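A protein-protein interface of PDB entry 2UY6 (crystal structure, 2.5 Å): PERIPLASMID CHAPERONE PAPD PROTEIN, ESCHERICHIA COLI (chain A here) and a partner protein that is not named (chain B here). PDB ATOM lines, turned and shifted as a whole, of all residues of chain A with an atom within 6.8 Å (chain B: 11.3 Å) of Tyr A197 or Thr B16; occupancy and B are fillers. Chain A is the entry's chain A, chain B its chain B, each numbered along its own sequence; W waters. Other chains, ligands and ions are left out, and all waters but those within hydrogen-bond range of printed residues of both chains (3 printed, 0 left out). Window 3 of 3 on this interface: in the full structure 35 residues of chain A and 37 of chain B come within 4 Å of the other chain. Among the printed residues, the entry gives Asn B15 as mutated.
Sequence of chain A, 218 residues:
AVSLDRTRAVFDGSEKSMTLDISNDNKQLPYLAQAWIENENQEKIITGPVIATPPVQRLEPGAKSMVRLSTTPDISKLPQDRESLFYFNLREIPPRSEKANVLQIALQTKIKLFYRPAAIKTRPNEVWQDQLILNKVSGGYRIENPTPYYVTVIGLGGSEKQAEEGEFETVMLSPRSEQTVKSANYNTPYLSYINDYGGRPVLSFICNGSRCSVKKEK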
ATOM      1  N   ARG A   6      16.268  27.346   5.542  1.00  0.00           N
ATOM      2  CA  ARG A   6      15.964  25.954   5.201  1.00  0.00           C
ATOM      3  C   ARG A   6      15.691  25.064   6.411  1.00  0.00           C
ATOM      4  O   ARG A   6      16.019  25.426   7.543  1.00  0.00           O
ATOM      5  CB  ARG A   6      17.090  25.326   4.375  1.00  0.00           C
ATOM      6  CG  ARG A   6      18.428  25.297   5.052  1.00  0.00           C
ATOM      7  CD  ARG A   6      19.303  26.376   4.485  1.00  0.00           C
ATOM      8  NE  ARG A   6      20.345  25.821   3.643  1.00  0.00           N
ATOM      9  CZ  ARG A   6      21.100  26.542   2.824  1.00  0.00           C
ATOM     10  NH1 ARG A   6      20.923  27.856   2.731  1.00  0.00           N
ATOM     11  NH2 ARG A   6      22.048  25.948   2.117  1.00  0.00           N
ATOM     12  N   THR A   7      15.100  23.896   6.160  1.00  0.00           N
ATOM     13  CA  THR A   7      14.761  22.950   7.220  1.00  0.00           C
ATOM     14  C   THR A   7      15.858  21.918   7.469  1.00  0.00           C
ATOM     15  O   THR A   7      15.820  21.167   8.439  1.00  0.00           O
ATOM     16  CB  THR A   7      13.420  22.235   6.902  1.00  0.00           C
ATOM     17  OG1 THR A   7      13.541  21.459   5.699  1.00  0.00           O
ATOM     18  CG2 THR A   7      12.325  23.267   6.695  1.00  0.00           C
ATOM     19  N   ARG A   8      16.831  21.881   6.570  1.00  0.00           N
ATOM     20  CA  ARG A   8      17.972  20.978   6.680  1.00  0.00           C
ATOM     21  C   ARG A   8      19.133  21.630   5.950  1.00  0.00           C
ATOM     22  O   ARG A   8      18.927  22.478   5.087  1.00  0.00           O
ATOM     23  CB  ARG A   8      17.666  19.620   6.046  1.00  0.00           C
ATOM     24  CG  ARG A   8      17.309  19.662   4.556  1.00  0.00           C
ATOM     25  CD  ARG A   8      16.306  18.545   4.253  1.00  0.00           C
ATOM     26  NE  ARG A   8      15.202  18.668   5.191  1.00  0.00           N
ATOM     27  CZ  ARG A   8      14.821  17.741   6.062  1.00  0.00           C
ATOM     28  NH1 ARG A   8      15.429  16.562   6.147  1.00  0.00           N
ATOM     29  NH2 ARG A   8      13.838  18.030   6.892  1.00  0.00           N
ATOM     30  N   ARG A 123      24.332  15.115  -7.164  1.00  0.00           N
ATOM     31  CA  ARG A 123      23.902  16.011  -8.233  1.00  0.00           C
ATOM     32  C   ARG A 123      22.564  16.643  -7.895  1.00  0.00           C
ATOM     33  O   ARG A 123      21.750  16.061  -7.190  1.00  0.00           O
ATOM     34  CB  ARG A 123      23.783  15.243  -9.547  1.00  0.00           C
ATOM     35  CG  ARG A 123      25.093  14.615 -10.000  1.00  0.00           C
ATOM     36  CD  ARG A 123      24.896  13.623 -11.158  1.00  0.00           C
ATOM     37  NE  ARG A 123      23.964  12.547 -10.819  1.00  0.00           N
ATOM     38  CZ  ARG A 123      23.728  11.480 -11.581  1.00  0.00           C
ATOM     39  NH1 ARG A 123      24.357  11.321 -12.745  1.00  0.00           N
ATOM     40  NH2 ARG A 123      22.852  10.572 -11.176  1.00  0.00           N
ATOM     41  N   PRO A 124      22.310  17.840  -8.420  1.00  0.00           N
ATOM     42  CA  PRO A 124      21.086  18.606  -8.207  1.00  0.00           C
ATOM     43  C   PRO A 124      19.798  17.903  -7.747  1.00  0.00           C
ATOM     44  O   PRO A 124      19.333  18.156  -6.637  1.00  0.00           O
ATOM     45  CB  PRO A 124      20.945  19.343  -9.517  1.00  0.00           C
ATOM     46  CG  PRO A 124      22.368  19.757  -9.735  1.00  0.00           C
ATOM     47  CD  PRO A 124      23.140  18.482  -9.453  1.00  0.00           C
ATOM     48  N   ASN A 125      19.191  17.042  -8.550  1.00  0.00           N
ATOM     49  CA  ASN A 125      17.963  16.403  -8.061  1.00  0.00           C
ATOM     50  C   ASN A 125      18.156  14.903  -7.883  1.00  0.00           C
ATOM     51  O   ASN A 125      17.223  14.128  -8.064  1.00  0.00           O
ATOM     52  CB  ASN A 125      16.797  16.636  -9.031  1.00  0.00           C
ATOM     53  CG  ASN A 125      16.322  18.073  -9.047  1.00  0.00           C
ATOM     54  OD1 ASN A 125      15.883  18.607  -8.026  1.00  0.00           O
ATOM     55  ND2 ASN A 125      16.400  18.709 -10.212  1.00  0.00           N
ATOM     56  N   GLU A 126      19.362  14.491  -7.521  1.00  0.00           N
ATOM     57  CA  GLU A 126      19.630  13.075  -7.377  1.00  0.00           C
ATOM     58  C   GLU A 126      18.791  12.414  -6.296  1.00  0.00           C
ATOM     59  O   GLU A 126      18.424  13.038  -5.290  1.00  0.00           O
ATOM     60  CB  GLU A 126      21.121  12.843  -7.124  1.00  0.00           C
ATOM     61  CG  GLU A 126      21.556  11.387  -7.241  1.00  0.00           C
ATOM     62  CD  GLU A 126      23.071  11.223  -7.256  1.00  0.00           C
ATOM     63  OE1 GLU A 126      23.544  10.075  -7.104  1.00  0.00           O
ATOM     64  OE2 GLU A 126      23.792  12.236  -7.430  1.00  0.00           O
ATOM     65  N   ILE A 194      11.800  12.750   3.225  1.00  0.00           N
ATOM     66  CA  ILE A 194      12.127  14.165   3.055  1.00  0.00           C
ATOM     67  C   ILE A 194      13.461  14.322   2.337  1.00  0.00           C
ATOM     68  O   ILE A 194      14.500  13.907   2.856  1.00  0.00           O
ATOM     69  CB  ILE A 194      12.236  14.884   4.400  1.00  0.00           C
ATOM     70  CG1 ILE A 194      11.008  14.573   5.264  1.00  0.00           C
ATOM     71  CG2 ILE A 194      12.365  16.374   4.160  1.00  0.00           C
ATOM     72  CD1 ILE A 194      10.965  15.340   6.593  1.00  0.00           C
ATOM     73  N   ASN A 195      13.447  14.923   1.152  1.00  0.00           N
ATOM     74  CA  ASN A 195      14.696  15.099   0.413  1.00  0.00           C
ATOM     75  C   ASN A 195      15.452  16.359   0.843  1.00  0.00           C
ATOM     76  O   ASN A 195      14.981  17.117   1.692  1.00  0.00           O
ATOM     77  CB  ASN A 195      14.451  15.110  -1.104  1.00  0.00           C
ATOM     78  CG  ASN A 195      13.599  16.276  -1.552  1.00  0.00           C
ATOM     79  OD1 ASN A 195      13.728  17.387  -1.041  1.00  0.00           O
ATOM     80  ND2 ASN A 195      12.733  16.034  -2.525  1.00  0.00           N
ATOM     81  N   ASP A 196      16.626  16.563   0.253  1.00  0.00           N
ATOM     82  CA  ASP A 196      17.484  17.704   0.575  1.00  0.00           C
ATOM     83  C   ASP A 196      16.756  19.047   0.556  1.00  0.00           C
ATOM     84  O   ASP A 196      17.035  19.912   1.376  1.00  0.00           O
ATOM     85  CB  ASP A 196      18.671  17.782  -0.407  1.00  0.00           C
ATOM     86  CG  ASP A 196      19.682  16.638  -0.239  1.00  0.00           C
ATOM     87  OD1 ASP A 196      19.554  15.819   0.699  1.00  0.00           O
ATOM     88  OD2 ASP A 196      20.626  16.568  -1.066  1.00  0.00           O
ATOM     89  N   TYR A 197      15.831  19.221  -0.387  1.00  0.00           N
ATOM     90  CA  TYR A 197      15.102  20.483  -0.540  1.00  0.00           C
ATOM     91  C   TYR A 197      13.889  20.655   0.373  1.00  0.00           C
ATOM     92  O   TYR A 197      13.237  21.704   0.357  1.00  0.00           O
ATOM     93  CB  TYR A 197      14.651  20.643  -1.996  1.00  0.00           C
ATOM     94  CG  TYR A 197      15.776  20.501  -3.004  1.00  0.00           C
ATOM     95  CD1 TYR A 197      16.131  19.256  -3.527  1.00  0.00           C
ATOM     96  CD2 TYR A 197      16.518  21.614  -3.400  1.00  0.00           C
ATOM     97  CE1 TYR A 197      17.207  19.129  -4.417  1.00  0.00           C
ATOM     98  CE2 TYR A 197      17.586  21.496  -4.278  1.00  0.00           C
ATOM     99  CZ  TYR A 197      17.928  20.259  -4.780  1.00  0.00           C
ATOM    100  OH  TYR A 197      19.009  20.174  -5.621  1.00  0.00           O
ATOM    101  N   GLY A 198      13.588  19.626   1.162  1.00  0.00           N
ATOM    102  CA  GLY A 198      12.442  19.682   2.050  1.00  0.00           C
ATOM    103  C   GLY A 198      11.218  19.029   1.424  1.00  0.00           C
ATOM    104  O   GLY A 198      10.161  18.957   2.051  1.00  0.00           O
ATOM    105  N   GLY A 199      11.362  18.557   0.186  1.00  0.00           N
ATOM    106  CA  GLY A 199      10.260  17.905  -0.495  1.00  0.00           C
ATOM    107  C   GLY A 199       9.980  16.538   0.089  1.00  0.00           C
ATOM    108  O   GLY A 199      10.860  15.913   0.678  1.00  0.00           O
ATOM    109  N   THR B  12      20.134  30.488 -20.061  1.00  0.00           N
ATOM    110  CA  THR B  12      19.670  29.417 -19.200  1.00  0.00           C
ATOM    111  C   THR B  12      19.412  29.996 -17.812  1.00  0.00           C
ATOM    112  O   THR B  12      20.295  30.632 -17.223  1.00  0.00           O
ATOM    113  CB  THR B  12      20.708  28.300 -19.108  1.00  0.00           C
ATOM    114  OG1 THR B  12      20.978  27.796 -20.421  1.00  0.00           O
ATOM    115  CG2 THR B  12      20.189  27.164 -18.238  1.00  0.00           C
ATOM    116  N   PHE B  13      18.194  29.795 -17.309  1.00  0.00           N
ATOM    117  CA  PHE B  13      17.812  30.302 -15.996  1.00  0.00           C
ATOM    118  C   PHE B  13      17.874  29.185 -14.968  1.00  0.00           C
ATOM    119  O   PHE B  13      17.367  28.089 -15.203  1.00  0.00           O
ATOM    120  CB  PHE B  13      16.399  30.893 -16.031  1.00  0.00           C
ATOM    121  CG  PHE B  13      16.210  31.961 -17.076  1.00  0.00           C
ATOM    122  CD1 PHE B  13      15.874  31.623 -18.387  1.00  0.00           C
ATOM    123  CD2 PHE B  13      16.380  33.304 -16.755  1.00  0.00           C
ATOM    124  CE1 PHE B  13      15.711  32.610 -19.360  1.00  0.00           C
ATOM    125  CE2 PHE B  13      16.219  34.297 -17.718  1.00  0.00           C
ATOM    126  CZ  PHE B  13      15.883  33.953 -19.022  1.00  0.00           C
ATOM    127  N   ASN B  14      18.505  29.469 -13.835  1.00  0.00           N
ATOM    128  CA  ASN B  14      18.625  28.479 -12.771  1.00  0.00           C
ATOM    129  C   ASN B  14      18.120  28.976 -11.426  1.00  0.00           C
ATOM    130  O   ASN B  14      18.293  30.143 -11.066  1.00  0.00           O
ATOM    131  CB  ASN B  14      20.077  28.043 -12.608  1.00  0.00           C
ATOM    132  CG  ASN B  14      20.566  27.241 -13.776  1.00  0.00           C
ATOM    133  OD1 ASN B  14      20.062  26.150 -14.035  1.00  0.00           O
ATOM    134  ND2 ASN B  14      21.551  27.774 -14.500  1.00  0.00           N
ATOM    135  N   ASN B  15      17.496  28.077 -10.679  1.00  0.00           N
ATOM    136  CA  ASN B  15      17.003  28.439  -9.366  1.00  0.00           C
ATOM    137  C   ASN B  15      16.747  27.169  -8.583  1.00  0.00           C
ATOM    138  O   ASN B  15      16.742  26.077  -9.134  1.00  0.00           O
ATOM    139  CB  ASN B  15      15.718  29.262  -9.479  1.00  0.00           C
ATOM    140  CG  ASN B  15      14.502  28.403  -9.729  1.00  0.00           C
ATOM    141  OD1 ASN B  15      14.031  27.703  -8.832  1.00  0.00           O
ATOM    142  ND2 ASN B  15      13.985  28.448 -10.946  1.00  0.00           N
ATOM    143  N   THR B  16      16.529  27.318  -7.292  1.00  0.00           N
ATOM    144  CA  THR B  16      16.278  26.167  -6.458  1.00  0.00           C
ATOM    145  C   THR B  16      15.127  26.505  -5.511  1.00  0.00           C
ATOM    146  O   THR B  16      14.936  27.666  -5.151  1.00  0.00           O
ATOM    147  CB  THR B  16      17.588  25.801  -5.719  1.00  0.00           C
ATOM    148  OG1 THR B  16      17.930  24.443  -6.021  1.00  0.00           O
ATOM    149  CG2 THR B  16      17.473  26.006  -4.230  1.00  0.00           C
ATOM    150  N   VAL B  17      14.330  25.508  -5.146  1.00  0.00           N
ATOM    151  CA  VAL B  17      13.213  25.744  -4.233  1.00  0.00           C
ATOM    152  C   VAL B  17      13.270  24.812  -3.023  1.00  0.00           C
ATOM    153  O   VAL B  17      13.424  23.591  -3.155  1.00  0.00           O
ATOM    154  CB  VAL B  17      11.846  25.552  -4.926  1.00  0.00           C
ATOM    155  CG1 VAL B  17      10.726  25.821  -3.929  1.00  0.00           C
ATOM    156  CG2 VAL B  17      11.716  26.498  -6.105  1.00  0.00           C
ATOM    157  N   VAL B  18      13.141  25.398  -1.841  1.00  0.00           N
ATOM    158  CA  VAL B  18      13.182  24.628  -0.613  1.00  0.00           C
ATOM    159  C   VAL B  18      12.025  24.999   0.299  1.00  0.00           C
ATOM    160  O   VAL B  18      11.395  26.043   0.134  1.00  0.00           O
ATOM    161  CB  VAL B  18      14.485  24.889   0.166  1.00  0.00           C
ATOM    162  CG1 VAL B  18      15.685  24.490  -0.672  1.00  0.00           C
ATOM    163  CG2 VAL B  18      14.549  26.364   0.578  1.00  0.00           C
ATOM    164  N   ASP B  19      11.763  24.125   1.262  1.00  0.00           N
ATOM    165  CA  ASP B  19      10.721  24.337   2.245  1.00  0.00           C
ATOM    166  C   ASP B  19      11.391  25.172   3.340  1.00  0.00           C
ATOM    167  O   ASP B  19      12.422  24.777   3.883  1.00  0.00           O
ATOM    168  CB  ASP B  19      10.274  22.994   2.802  1.00  0.00           C
ATOM    169  CG  ASP B  19       9.010  23.097   3.612  1.00  0.00           C
ATOM    170  OD1 ASP B  19       8.795  22.227   4.481  1.00  0.00           O
ATOM    171  OD2 ASP B  19       8.229  24.038   3.373  1.00  0.00           O
ATOM    172  N   ALA B  20      10.820  26.330   3.646  1.00  0.00           N
ATOM    173  CA  ALA B  20      11.397  27.218   4.650  1.00  0.00           C
ATOM    174  C   ALA B  20      10.905  26.890   6.056  1.00  0.00           C
ATOM    175  O   ALA B  20       9.782  26.428   6.229  1.00  0.00           O
ATOM    176  CB  ALA B  20      11.070  28.685   4.303  1.00  0.00           C
ATOM    177  N   PRO B  21      11.749  27.116   7.079  1.00  0.00           N
ATOM    178  CA  PRO B  21      11.354  26.834   8.463  1.00  0.00           C
ATOM    179  C   PRO B  21      10.406  27.946   8.886  1.00  0.00           C
ATOM    180  O   PRO B  21      10.398  29.020   8.278  1.00  0.00           O
ATOM    181  CB  PRO B  21      12.669  26.904   9.237  1.00  0.00           C
ATOM    182  CG  PRO B  21      13.746  26.893   8.179  1.00  0.00           C
ATOM    183  CD  PRO B  21      13.126  27.625   7.034  1.00  0.00           C
ATOM    184  N   ASP B  62       5.057  26.771   5.462  1.00  0.00           N
ATOM    185  CA  ASP B  62       3.864  26.024   5.100  1.00  0.00           C
ATOM    186  C   ASP B  62       3.374  25.477   6.422  1.00  0.00           C
ATOM    187  O   ASP B  62       4.014  24.611   7.014  1.00  0.00           O
ATOM    188  CB  ASP B  62       4.207  24.884   4.144  1.00  0.00           C
ATOM    189  N   TYR B 162      13.090  20.593  13.314  1.00  0.00           N
ATOM    190  CA  TYR B 162      12.668  19.920  12.099  1.00  0.00           C
ATOM    191  C   TYR B 162      13.347  18.596  11.830  1.00  0.00           C
ATOM    192  O   TYR B 162      14.522  18.404  12.129  1.00  0.00           O
ATOM    193  CB  TYR B 162      12.885  20.830  10.891  1.00  0.00           C
ATOM    194  CG  TYR B 162      12.149  22.128  11.008  1.00  0.00           C
ATOM    195  CD1 TYR B 162      12.581  23.113  11.898  1.00  0.00           C
ATOM    196  CD2 TYR B 162      10.982  22.354  10.286  1.00  0.00           C
ATOM    197  CE1 TYR B 162      11.866  24.291  12.071  1.00  0.00           C
ATOM    198  CE2 TYR B 162      10.250  23.535  10.452  1.00  0.00           C
ATOM    199  CZ  TYR B 162      10.699  24.495  11.347  1.00  0.00           C
ATOM    200  OH  TYR B 162       9.979  25.653  11.537  1.00  0.00           O
ATOM    201  N   GLN B 163      12.582  17.669  11.273  1.00  0.00           N
ATOM    202  CA  GLN B 163      13.141  16.385  10.898  1.00  0.00           C
ATOM    203  C   GLN B 163      13.281  16.426   9.395  1.00  0.00           C
ATOM    204  O   GLN B 163      12.678  17.353   8.815  1.00  0.00           O
ATOM    205  CB  GLN B 163      12.225  15.256  11.329  1.00  0.00           C
ATOM    206  CG  GLN B 163      12.463  14.904  12.761  1.00  0.00           C
ATOM    207  CD  GLN B 163      11.528  13.855  13.245  1.00  0.00           C
ATOM    208  OE1 GLN B 163      10.311  14.063  13.273  1.00  0.00           O
ATOM    209  NE2 GLN B 163      12.075  12.708  13.634  1.00  0.00           N
ATOM    210  OXT GLN B 163      13.982  15.565   8.834  1.00  0.00           O
HETATM  211  O   HOH W   1      10.033  19.758   5.114  1.00  0.00           O
HETATM  212  O   HOH W   2      16.260  18.638   9.912  1.00  0.00           O
HETATM  213  O   HOH W   3      14.052  22.800   3.633  1.00  0.00           O
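The chain-end carboxylate (OXT) of Gln B163 is in salt-bridge range of the guanidinium group (NH2) of Arg A8 (3.1 Å). The backbone NH (N) of Asp B19 is in hydrogen-bond range of the backbone carbonyl oxygen (O) of Tyr A197, at 3.0 Å.
OG1 of Thr A7 lies within hydrogen-bond range of NE of Arg A8 (3.3 Å). The side-chain amide oxygen of Asn A195 sits at hydrogen-bond distance from the backbone NH of Tyr A197.
Among the printed residues, pairs that only touch across the chains: Arg A6 with Asp B19 (3.96 Å), Arg A6 with Pro B21 (2.8 Å), Thr A7 with Asp B19 (3.2 Å), Thr A7 with Ala B20 (3.9 Å), Thr A7 with Pro B21 (3.9 Å), Thr A7 with Tyr B162 (3.8 Å), Ile A194 with Gln B163 (3.5 Å), Tyr A197 with Thr B16 (3.4 Å), Tyr A197 with Val B17 (3.4 Å) and Tyr A197 with Val B18 (3.1 Å).
Of chain A, only Tyr A197 (3.4 Å) comes within 4 Å of Thr B16. No residue of chain B comes within 4 Å of Asn A125. No residue of chain B comes within 4 Å of Asn A195. Gly A198 touches none of the printed residues of chain B. No residue of chain B comes within 4 Å of Gly A199. Of the printed residues of chain A, Val B17 touches Tyr A197. Of the printed residues of chain B, Arg A8 touches Gln B163. Of the printed residues of chain A, Val B18 touches Tyr A197 (3.1 Å). Of the printed residues of chain A, Pro B21 touches Arg A6 and Thr A7. Asp B62 touches none of the printed residues of chain A. Asn B14 touches none of the printed residues of chain A. The nearest residue of chain B that does not touch Tyr A197 is Ala B20 (6.2 Å). The nearest residue of chain A that does not touch Thr B16 is Pro A124 (6.5 Å). The nearest printed residue of chain A that does not touch Val B17 is Gly A198 (5.9 Å).
Hydrophobic or aromatic side chains of chain A within 4 Å of the printed part of chain B: Ile A194 and Tyr A197. Of the 13 printed residues of chain B, 8 touch a printed residue of chain A. Hydrophobic or aromatic side chains of chain B that line the printed part of chain A: Val B18, Pro B21 and Tyr B162. Among the printed residues, 12 pairs touch across the chains. Among the printed residues, no Asp or Glu carboxylate lies within 4 Å of a Lys or Arg side-chain nitrogen of the other chain.
Water W3 bridges OG1 of Thr A7 (2.5 Å) and O of Asp B19 (2.6 Å). Water W2 bridges the backbone carbonyl oxygen of Tyr B162 (2.8 Å) and the backbone carbonyl oxygen of Thr A7 (3.0 Å). Water W1 lies within hydrogen-bond range of OD1 of Asp B19 (2.8 Å) and O of Gly A198 (3.2 Å).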
